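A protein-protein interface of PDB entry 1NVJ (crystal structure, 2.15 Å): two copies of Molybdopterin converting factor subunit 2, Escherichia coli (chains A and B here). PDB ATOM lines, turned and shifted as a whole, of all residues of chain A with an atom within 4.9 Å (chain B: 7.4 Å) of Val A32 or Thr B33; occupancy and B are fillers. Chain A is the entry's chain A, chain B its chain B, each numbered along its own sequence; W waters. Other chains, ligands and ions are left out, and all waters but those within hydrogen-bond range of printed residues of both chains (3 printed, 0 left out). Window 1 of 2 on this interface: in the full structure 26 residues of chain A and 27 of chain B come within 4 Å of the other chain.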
ATOM      1  N   LEU A  22     -14.542  -3.886   5.984  1.00  0.00           N
ATOM      2  CA  LEU A  22     -14.454  -2.869   4.949  1.00  0.00           C
ATOM      3  C   LEU A  22     -13.337  -1.889   5.236  1.00  0.00           C
ATOM      4  O   LEU A  22     -12.560  -1.549   4.348  1.00  0.00           O
ATOM      5  CB  LEU A  22     -15.810  -2.175   4.822  1.00  0.00           C
ATOM      6  CG  LEU A  22     -15.968  -1.173   3.704  1.00  0.00           C
ATOM      7  CD1 LEU A  22     -15.819  -1.871   2.386  1.00  0.00           C
ATOM      8  CD2 LEU A  22     -17.317  -0.529   3.860  1.00  0.00           C
ATOM      9  N   ALA A  30     -10.329   6.173   2.948  1.00  0.00           N
ATOM     10  CA  ALA A  30     -11.614   6.796   2.709  1.00  0.00           C
ATOM     11  C   ALA A  30     -12.644   5.716   2.515  1.00  0.00           C
ATOM     12  O   ALA A  30     -12.554   4.919   1.581  1.00  0.00           O
ATOM     13  CB  ALA A  30     -11.563   7.743   1.454  1.00  0.00           C
ATOM     14  N   VAL A  31     -13.663   5.720   3.361  1.00  0.00           N
ATOM     15  CA  VAL A  31     -14.641   4.641   3.422  1.00  0.00           C
ATOM     16  C   VAL A  31     -16.010   5.282   3.255  1.00  0.00           C
ATOM     17  O   VAL A  31     -16.404   6.118   4.062  1.00  0.00           O
ATOM     18  CB  VAL A  31     -14.556   3.912   4.773  1.00  0.00           C
ATOM     19  CG1 VAL A  31     -15.584   2.749   4.847  1.00  0.00           C
ATOM     20  CG2 VAL A  31     -13.166   3.427   5.036  1.00  0.00           C
ATOM     21  N   VAL A  32     -16.704   4.933   2.173  1.00  0.00           N
ATOM     22  CA  VAL A  32     -18.067   5.398   1.928  1.00  0.00           C
ATOM     23  C   VAL A  32     -19.037   4.238   2.061  1.00  0.00           C
ATOM     24  O   VAL A  32     -18.820   3.164   1.486  1.00  0.00           O
ATOM     25  CB  VAL A  32     -18.197   5.969   0.505  1.00  0.00           C
ATOM     26  CG1 VAL A  32     -19.669   6.175   0.123  1.00  0.00           C
ATOM     27  CG2 VAL A  32     -17.383   7.263   0.359  1.00  0.00           C
ATOM     28  N   THR A  33     -20.132   4.434   2.772  1.00  0.00           N
ATOM     29  CA  THR A  33     -21.202   3.453   2.705  1.00  0.00           C
ATOM     30  C   THR A  33     -22.520   4.069   2.292  1.00  0.00           C
ATOM     31  O   THR A  33     -22.796   5.234   2.545  1.00  0.00           O
ATOM     32  CB  THR A  33     -21.403   2.724   4.023  1.00  0.00           C
ATOM     33  OG1 THR A  33     -22.022   3.590   5.013  1.00  0.00           O
ATOM     34  CG2 THR A  33     -20.084   2.323   4.621  1.00  0.00           C
ATOM     35  N   PHE A  34     -23.324   3.235   1.652  1.00  0.00           N
ATOM     36  CA  PHE A  34     -24.708   3.521   1.416  1.00  0.00           C
ATOM     37  C   PHE A  34     -25.564   2.380   1.928  1.00  0.00           C
ATOM     38  O   PHE A  34     -25.257   1.213   1.698  1.00  0.00           O
ATOM     39  CB  PHE A  34     -24.980   3.714  -0.070  1.00  0.00           C
ATOM     40  CG  PHE A  34     -26.420   3.913  -0.355  1.00  0.00           C
ATOM     41  CD1 PHE A  34     -26.974   5.157  -0.242  1.00  0.00           C
ATOM     42  CD2 PHE A  34     -27.237   2.832  -0.664  1.00  0.00           C
ATOM     43  CE1 PHE A  34     -28.338   5.344  -0.433  1.00  0.00           C
ATOM     44  CE2 PHE A  34     -28.584   3.026  -0.893  1.00  0.00           C
ATOM     45  CZ  PHE A  34     -29.129   4.289  -0.762  1.00  0.00           C
ATOM     46  N   VAL A  97     -23.918  -0.980   0.340  1.00  0.00           N
ATOM     47  CA  VAL A  97     -22.749  -0.895  -0.550  1.00  0.00           C
ATOM     48  C   VAL A  97     -21.668  -0.154   0.192  1.00  0.00           C
ATOM     49  O   VAL A  97     -21.882   0.968   0.646  1.00  0.00           O
ATOM     50  CB  VAL A  97     -23.074  -0.110  -1.816  1.00  0.00           C
ATOM     51  CG1 VAL A  97     -21.801   0.233  -2.628  1.00  0.00           C
ATOM     52  CG2 VAL A  97     -24.073  -0.865  -2.655  1.00  0.00           C
ATOM     53  N   GLY A  98     -20.503  -0.772   0.294  1.00  0.00           N
ATOM     54  CA  GLY A  98     -19.371  -0.188   1.007  1.00  0.00           C
ATOM     55  C   GLY A  98     -18.204  -0.124   0.056  1.00  0.00           C
ATOM     56  O   GLY A  98     -17.873  -1.137  -0.540  1.00  0.00           O
ATOM     57  N   VAL A  99     -17.638   1.065  -0.129  1.00  0.00           N
ATOM     58  CA  VAL A  99     -16.482   1.246  -1.002  1.00  0.00           C
ATOM     59  C   VAL A  99     -15.382   2.036  -0.289  1.00  0.00           C
ATOM     60  O   VAL A  99     -15.659   2.994   0.450  1.00  0.00           O
ATOM     61  CB  VAL A  99     -16.872   2.007  -2.280  1.00  0.00           C
ATOM     62  CG1 VAL A  99     -15.684   2.129  -3.216  1.00  0.00           C
ATOM     63  CG2 VAL A  99     -18.036   1.310  -2.990  1.00  0.00           C
ATOM     64  N   ARG A 104     -11.281  10.284  -1.617  1.00  0.00           N
ATOM     65  CA  ARG A 104     -12.714  10.519  -1.379  1.00  0.00           C
ATOM     66  C   ARG A 104     -13.557  10.483  -2.636  1.00  0.00           C
ATOM     67  O   ARG A 104     -14.591   9.833  -2.698  1.00  0.00           O
ATOM     68  CB  ARG A 104     -12.864  11.921  -0.754  1.00  0.00           C
ATOM     69  CG  ARG A 104     -13.817  12.015   0.318  1.00  0.00           C
ATOM     70  CD  ARG A 104     -13.483  12.994   1.384  1.00  0.00           C
ATOM     71  NE  ARG A 104     -13.702  14.382   1.009  1.00  0.00           N
ATOM     72  CZ  ARG A 104     -12.824  15.353   1.249  1.00  0.00           C
ATOM     73  NH1 ARG A 104     -11.677  15.086   1.819  1.00  0.00           N
ATOM     74  NH2 ARG A 104     -13.095  16.600   0.911  1.00  0.00           N
ATOM     75  N   ALA A 107     -14.093   6.915  -4.002  1.00  0.00           N
ATOM     76  CA  ALA A 107     -15.016   6.096  -3.260  1.00  0.00           C
ATOM     77  C   ALA A 107     -16.493   6.571  -3.391  1.00  0.00           C
ATOM     78  O   ALA A 107     -17.398   5.756  -3.548  1.00  0.00           O
ATOM     79  CB  ALA A 107     -14.570   6.024  -1.811  1.00  0.00           C
ATOM     80  N   PHE A 108     -16.740   7.870  -3.353  1.00  0.00           N
ATOM     81  CA  PHE A 108     -18.093   8.397  -3.593  1.00  0.00           C
ATOM     82  C   PHE A 108     -18.616   8.100  -5.025  1.00  0.00           C
ATOM     83  O   PHE A 108     -19.754   7.655  -5.188  1.00  0.00           O
ATOM     84  CB  PHE A 108     -18.138   9.906  -3.350  1.00  0.00           C
ATOM     85  CG  PHE A 108     -18.344  10.285  -1.904  1.00  0.00           C
ATOM     86  CD1 PHE A 108     -17.346  10.936  -1.197  1.00  0.00           C
ATOM     87  CD2 PHE A 108     -19.544  10.011  -1.260  1.00  0.00           C
ATOM     88  CE1 PHE A 108     -17.537  11.297   0.101  1.00  0.00           C
ATOM     89  CE2 PHE A 108     -19.735  10.365   0.061  1.00  0.00           C
ATOM     90  CZ  PHE A 108     -18.761  11.004   0.746  1.00  0.00           C
ATOM     91  N   VAL B  15     -17.880   3.501  14.381  1.00  0.00           N
ATOM     92  CA  VAL B  15     -18.966   3.661  13.422  1.00  0.00           C
ATOM     93  C   VAL B  15     -20.126   2.789  13.789  1.00  0.00           C
ATOM     94  O   VAL B  15     -21.273   3.162  13.537  1.00  0.00           O
ATOM     95  CB  VAL B  15     -18.566   3.299  11.984  1.00  0.00           C
ATOM     96  CG1 VAL B  15     -19.801   3.227  11.068  1.00  0.00           C
ATOM     97  CG2 VAL B  15     -17.563   4.317  11.430  1.00  0.00           C
ATOM     98  N   GLU B  18     -22.265   4.581  16.175  1.00  0.00           N
ATOM     99  CA  GLU B  18     -22.920   5.771  15.633  1.00  0.00           C
ATOM    100  C   GLU B  18     -24.009   5.475  14.624  1.00  0.00           C
ATOM    101  O   GLU B  18     -24.974   6.241  14.492  1.00  0.00           O
ATOM    102  CB  GLU B  18     -21.900   6.648  14.933  1.00  0.00           C
ATOM    103  CG  GLU B  18     -20.786   7.139  15.818  1.00  0.00           C
ATOM    104  CD  GLU B  18     -21.254   8.012  16.957  1.00  0.00           C
ATOM    105  OE1 GLU B  18     -22.209   8.768  16.792  1.00  0.00           O
ATOM    106  OE2 GLU B  18     -20.644   7.928  18.029  1.00  0.00           O
ATOM    107  N   TYR B  19     -23.854   4.373  13.895  1.00  0.00           N
ATOM    108  CA  TYR B  19     -24.706   4.099  12.745  1.00  0.00           C
ATOM    109  C   TYR B  19     -26.172   3.853  13.134  1.00  0.00           C
ATOM    110  O   TYR B  19     -27.057   4.385  12.464  1.00  0.00           O
ATOM    111  CB  TYR B  19     -24.138   2.960  11.865  1.00  0.00           C
ATOM    112  CG  TYR B  19     -25.053   2.587  10.735  1.00  0.00           C
ATOM    113  CD1 TYR B  19     -24.905   3.148   9.470  1.00  0.00           C
ATOM    114  CD2 TYR B  19     -26.102   1.689  10.942  1.00  0.00           C
ATOM    115  CE1 TYR B  19     -25.790   2.816   8.430  1.00  0.00           C
ATOM    116  CE2 TYR B  19     -26.976   1.359   9.933  1.00  0.00           C
ATOM    117  CZ  TYR B  19     -26.826   1.924   8.680  1.00  0.00           C
ATOM    118  OH  TYR B  19     -27.706   1.555   7.677  1.00  0.00           O
ATOM    119  N   LEU B  22     -28.097   6.909  13.553  1.00  0.00           N
ATOM    120  CA  LEU B  22     -28.146   7.670  12.312  1.00  0.00           C
ATOM    121  C   LEU B  22     -29.245   7.122  11.425  1.00  0.00           C
ATOM    122  O   LEU B  22     -29.956   7.883  10.764  1.00  0.00           O
ATOM    123  CB  LEU B  22     -26.776   7.668  11.613  1.00  0.00           C
ATOM    124  CG  LEU B  22     -26.682   8.347  10.256  1.00  0.00           C
ATOM    125  CD1 LEU B  22     -26.840   9.852  10.386  1.00  0.00           C
ATOM    126  CD2 LEU B  22     -25.371   7.977   9.582  1.00  0.00           C
ATOM    127  N   VAL B  31     -29.162   6.170   3.570  1.00  0.00           N
ATOM    128  CA  VAL B  31     -28.147   6.479   4.589  1.00  0.00           C
ATOM    129  C   VAL B  31     -26.762   6.414   3.977  1.00  0.00           C
ATOM    130  O   VAL B  31     -26.350   5.366   3.481  1.00  0.00           O
ATOM    131  CB  VAL B  31     -28.177   5.475   5.734  1.00  0.00           C
ATOM    132  CG1 VAL B  31     -27.183   5.910   6.862  1.00  0.00           C
ATOM    133  CG2 VAL B  31     -29.586   5.336   6.277  1.00  0.00           C
ATOM    134  N   VAL B  32     -26.051   7.531   4.028  1.00  0.00           N
ATOM    135  CA  VAL B  32     -24.682   7.638   3.517  1.00  0.00           C
ATOM    136  C   VAL B  32     -23.751   7.944   4.670  1.00  0.00           C
ATOM    137  O   VAL B  32     -24.051   8.832   5.486  1.00  0.00           O
ATOM    138  CB  VAL B  32     -24.560   8.743   2.432  1.00  0.00           C
ATOM    139  CG1 VAL B  32     -23.092   9.049   2.094  1.00  0.00           C
ATOM    140  CG2 VAL B  32     -25.293   8.327   1.189  1.00  0.00           C
ATOM    141  N   THR B  33     -22.652   7.194   4.773  1.00  0.00           N
ATOM    142  CA  THR B  33     -21.556   7.598   5.628  1.00  0.00           C
ATOM    143  C   THR B  33     -20.232   7.726   4.893  1.00  0.00           C
ATOM    144  O   THR B  33     -20.003   7.091   3.888  1.00  0.00           O
ATOM    145  CB  THR B  33     -21.340   6.647   6.831  1.00  0.00           C
ATOM    146  OG1 THR B  33     -20.723   5.433   6.402  1.00  0.00           O
ATOM    147  CG2 THR B  33     -22.671   6.207   7.473  1.00  0.00           C
ATOM    148  N   PHE B  34     -19.376   8.571   5.452  1.00  0.00           N
ATOM    149  CA  PHE B  34     -17.988   8.682   5.071  1.00  0.00           C
ATOM    150  C   PHE B  34     -17.158   8.631   6.316  1.00  0.00           C
ATOM    151  O   PHE B  34     -17.428   9.350   7.300  1.00  0.00           O
ATOM    152  CB  PHE B  34     -17.696  10.024   4.382  1.00  0.00           C
ATOM    153  CG  PHE B  34     -16.271  10.191   4.074  1.00  0.00           C
ATOM    154  CD1 PHE B  34     -15.722   9.524   2.996  1.00  0.00           C
ATOM    155  CD2 PHE B  34     -15.443  10.880   4.935  1.00  0.00           C
ATOM    156  CE1 PHE B  34     -14.370   9.592   2.738  1.00  0.00           C
ATOM    157  CE2 PHE B  34     -14.109  10.956   4.676  1.00  0.00           C
ATOM    158  CZ  PHE B  34     -13.563  10.313   3.578  1.00  0.00           C
ATOM    159  N   THR B  35     -16.138   7.794   6.285  1.00  0.00           N
ATOM    160  CA  THR B  35     -15.123   7.773   7.318  1.00  0.00           C
ATOM    161  C   THR B  35     -13.782   8.100   6.703  1.00  0.00           C
ATOM    162  O   THR B  35     -13.368   7.486   5.716  1.00  0.00           O
ATOM    163  CB  THR B  35     -15.078   6.421   8.054  1.00  0.00           C
ATOM    164  OG1 THR B  35     -16.392   6.100   8.600  1.00  0.00           O
ATOM    165  CG2 THR B  35     -14.139   6.550   9.290  1.00  0.00           C
ATOM    166  N   PHE B  96     -15.991  11.333  10.719  1.00  0.00           N
ATOM    167  CA  PHE B  96     -17.176  10.588  10.362  1.00  0.00           C
ATOM    168  C   PHE B  96     -18.285  11.590  10.018  1.00  0.00           C
ATOM    169  O   PHE B  96     -18.589  12.487  10.799  1.00  0.00           O
ATOM    170  CB  PHE B  96     -17.624   9.719  11.545  1.00  0.00           C
ATOM    171  CG  PHE B  96     -18.878   8.962  11.286  1.00  0.00           C
ATOM    172  CD1 PHE B  96     -18.867   7.856  10.457  1.00  0.00           C
ATOM    173  CD2 PHE B  96     -20.078   9.361  11.858  1.00  0.00           C
ATOM    174  CE1 PHE B  96     -20.016   7.143  10.222  1.00  0.00           C
ATOM    175  CE2 PHE B  96     -21.236   8.678  11.609  1.00  0.00           C
ATOM    176  CZ  PHE B  96     -21.215   7.562  10.784  1.00  0.00           C
ATOM    177  N   VAL B  97     -18.856  11.443   8.837  1.00  0.00           N
ATOM    178  CA  VAL B  97     -20.022  12.195   8.438  1.00  0.00           C
ATOM    179  C   VAL B  97     -21.082  11.220   8.019  1.00  0.00           C
ATOM    180  O   VAL B  97     -20.862  10.381   7.129  1.00  0.00           O
ATOM    181  CB  VAL B  97     -19.696  13.143   7.273  1.00  0.00           C
ATOM    182  CG1 VAL B  97     -20.939  13.687   6.649  1.00  0.00           C
ATOM    183  CG2 VAL B  97     -18.836  14.285   7.768  1.00  0.00           C
ATOM    184  N   GLY B  98     -22.234  11.317   8.657  1.00  0.00           N
ATOM    185  CA  GLY B  98     -23.383  10.533   8.274  1.00  0.00           C
ATOM    186  C   GLY B  98     -24.556  11.440   7.940  1.00  0.00           C
ATOM    187  O   GLY B  98     -24.836  12.383   8.659  1.00  0.00           O
ATOM    188  N   VAL B  99     -25.261  11.110   6.873  1.00  0.00           N
ATOM    189  CA  VAL B  99     -26.363  11.890   6.384  1.00  0.00           C
ATOM    190  C   VAL B  99     -27.425  10.930   5.930  1.00  0.00           C
ATOM    191  O   VAL B  99     -27.123   9.854   5.415  1.00  0.00           O
ATOM    192  CB  VAL B  99     -25.967  12.730   5.152  1.00  0.00           C
ATOM    193  CG1 VAL B  99     -27.164  13.523   4.677  1.00  0.00           C
ATOM    194  CG2 VAL B  99     -24.776  13.680   5.458  1.00  0.00           C
ATOM    195  N   ALA B 107     -28.445  12.246  -0.343  1.00  0.00           N
ATOM    196  CA  ALA B 107     -27.554  11.817   0.748  1.00  0.00           C
ATOM    197  C   ALA B 107     -26.087  11.838   0.268  1.00  0.00           C
ATOM    198  O   ALA B 107     -25.223  12.322   0.966  1.00  0.00           O
ATOM    199  CB  ALA B 107     -27.940  10.427   1.283  1.00  0.00           C
ATOM    200  N   PHE B 108     -25.840  11.333  -0.932  1.00  0.00           N
ATOM    201  CA  PHE B 108     -24.504  11.293  -1.515  1.00  0.00           C
ATOM    202  C   PHE B 108     -23.922  12.703  -1.717  1.00  0.00           C
ATOM    203  O   PHE B 108     -22.794  12.988  -1.312  1.00  0.00           O
ATOM    204  CB  PHE B 108     -24.530  10.537  -2.844  1.00  0.00           C
ATOM    205  CG  PHE B 108     -24.252   9.064  -2.714  1.00  0.00           C
ATOM    206  CD1 PHE B 108     -25.176   8.127  -3.152  1.00  0.00           C
ATOM    207  CD2 PHE B 108     -23.070   8.618  -2.150  1.00  0.00           C
ATOM    208  CE1 PHE B 108     -24.930   6.779  -3.023  1.00  0.00           C
ATOM    209  CE2 PHE B 108     -22.818   7.265  -2.007  1.00  0.00           C
ATOM    210  CZ  PHE B 108     -23.749   6.340  -2.436  1.00  0.00           C
ATOM    211  N   GLY B 111     -23.404  14.487   1.776  1.00  0.00           N
ATOM    212  CA  GLY B 111     -22.257  13.890   2.438  1.00  0.00           C
ATOM    213  C   GLY B 111     -20.946  14.452   1.906  1.00  0.00           C
ATOM    214  O   GLY B 111     -20.043  14.786   2.675  1.00  0.00           O
ATOM    215  N   GLN B 112     -20.845  14.570   0.583  1.00  0.00           N
ATOM    216  CA  GLN B 112     -19.658  15.160  -0.050  1.00  0.00           C
ATOM    217  C   GLN B 112     -19.489  16.638   0.211  1.00  0.00           C
ATOM    218  O   GLN B 112     -18.380  17.107   0.437  1.00  0.00           O
ATOM    219  CB  GLN B 112     -19.684  14.930  -1.561  1.00  0.00           C
ATOM    220  CG  GLN B 112     -19.251  13.537  -1.942  1.00  0.00           C
ATOM    221  CD  GLN B 112     -19.411  13.286  -3.401  1.00  0.00           C
ATOM    222  OE1 GLN B 112     -20.513  13.018  -3.857  1.00  0.00           O
ATOM    223  NE2 GLN B 112     -18.330  13.404  -4.146  1.00  0.00           N
HETATM  224  O   HOH W   1     -16.392  14.822  -0.351  1.00  0.00           O
HETATM  225  O   HOH W   2     -24.788   3.561   5.172  1.00  0.00           O
HETATM  226  O   HOH W   3     -18.039   5.084   6.508  1.00  0.00           O
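Printed residues of chain B within 4 Å of Ala A30: Phe B34 and Thr B35.
Val A32 touches three residues of chain B.
Of chain A, only Val A31, Val A32 and Thr A33 come within 4 Å of Thr B33.
Of the printed residues of chain A, Gln B112 touches Phe A108.
The nearest printed residue of chain A that does not touch Phe B34 is Thr A33 (5.0 Å).
Val A31 touches Phe B34, and with the chains exchanged Phe A34 touches Val B31.
Val A32 touches Phe B34, and with the chains exchanged Phe A34 touches Val B32.
Thr B33 touches its own counterpart, Thr A33.
Phe A34 touches Phe B108, and with the chains exchanged Phe A108 touches Phe B34.
Of the 18 pairs that touch across the chains among the printed residues, 12 have their exchanged pair printed and touching as well.
N of Val A32 is in hydrogen-bond range of O of Val A99, 2.8 Å away.
O of Phe B108 lies close to OE1 of Gln B112 (3.4 Å).
The backbone NH (N) of Val B32 sits at hydrogen-bond distance from the backbone carbonyl oxygen (O) of Val B99, 2.9 Å away.
N of Phe B34 lies within hydrogen-bond range of O of Val B97, 2.9 Å away.
The backbone NH (N) of Phe A34 sits at hydrogen-bond distance from the backbone carbonyl oxygen (O) of Val A97.
The backbone carbonyl oxygen (O) of Val A31 lies within hydrogen-bond range of the backbone NH (N) of Thr B35 (2.8 Å).
OG1 of Thr B33 is in hydrogen-bond range of OG1 of Thr A33, at 2.6 Å.
Water W3 lies within hydrogen-bond range of the side-chain hydroxyl of Thr B33 (2.7 Å), the side-chain hydroxyl of Thr B35 (2.8 Å) and the backbone carbonyl oxygen of Val A31 (3.1 Å).
Water W2 bridges OG1 of Thr A33 (2.8 Å) and O of Val B31 (2.9 Å).
Water W1 lies within hydrogen-bond range of NE of Arg A104 (3.0 Å) and O of Gln B112 (3.1 Å).
CA of Ala A30 touches O of Thr B35, 3.5 Å away.
O of Val A31 touches O of Thr B33, 3.7 Å away.
Val A32 touches Phe B34 (CG2 to CD1, 3.9 Å).
Thr A33 touches Val B31 (O to O, 3.7 Å).
CA of Phe A34 touches O of Val B31, 3.2 Å away.
Phe A34 touches Val B32.
Phe B108 touches Phe A34.
CZ of Phe B34 touches CD of Arg A104, at 3.5 Å.
Phe A108 touches Phe B108.
Gln B112 touches Phe A108 (CG to CD1, 3.3 Å).
Of the 12 printed residues of chain A, 7 touch a printed residue of chain B.
Among the printed residues, 18 pairs touch across the chains.
Among the printed residues, no Asp or Glu carboxylate lies within 4 Å of a Lys or Arg side-chain nitrogen of the other chain.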
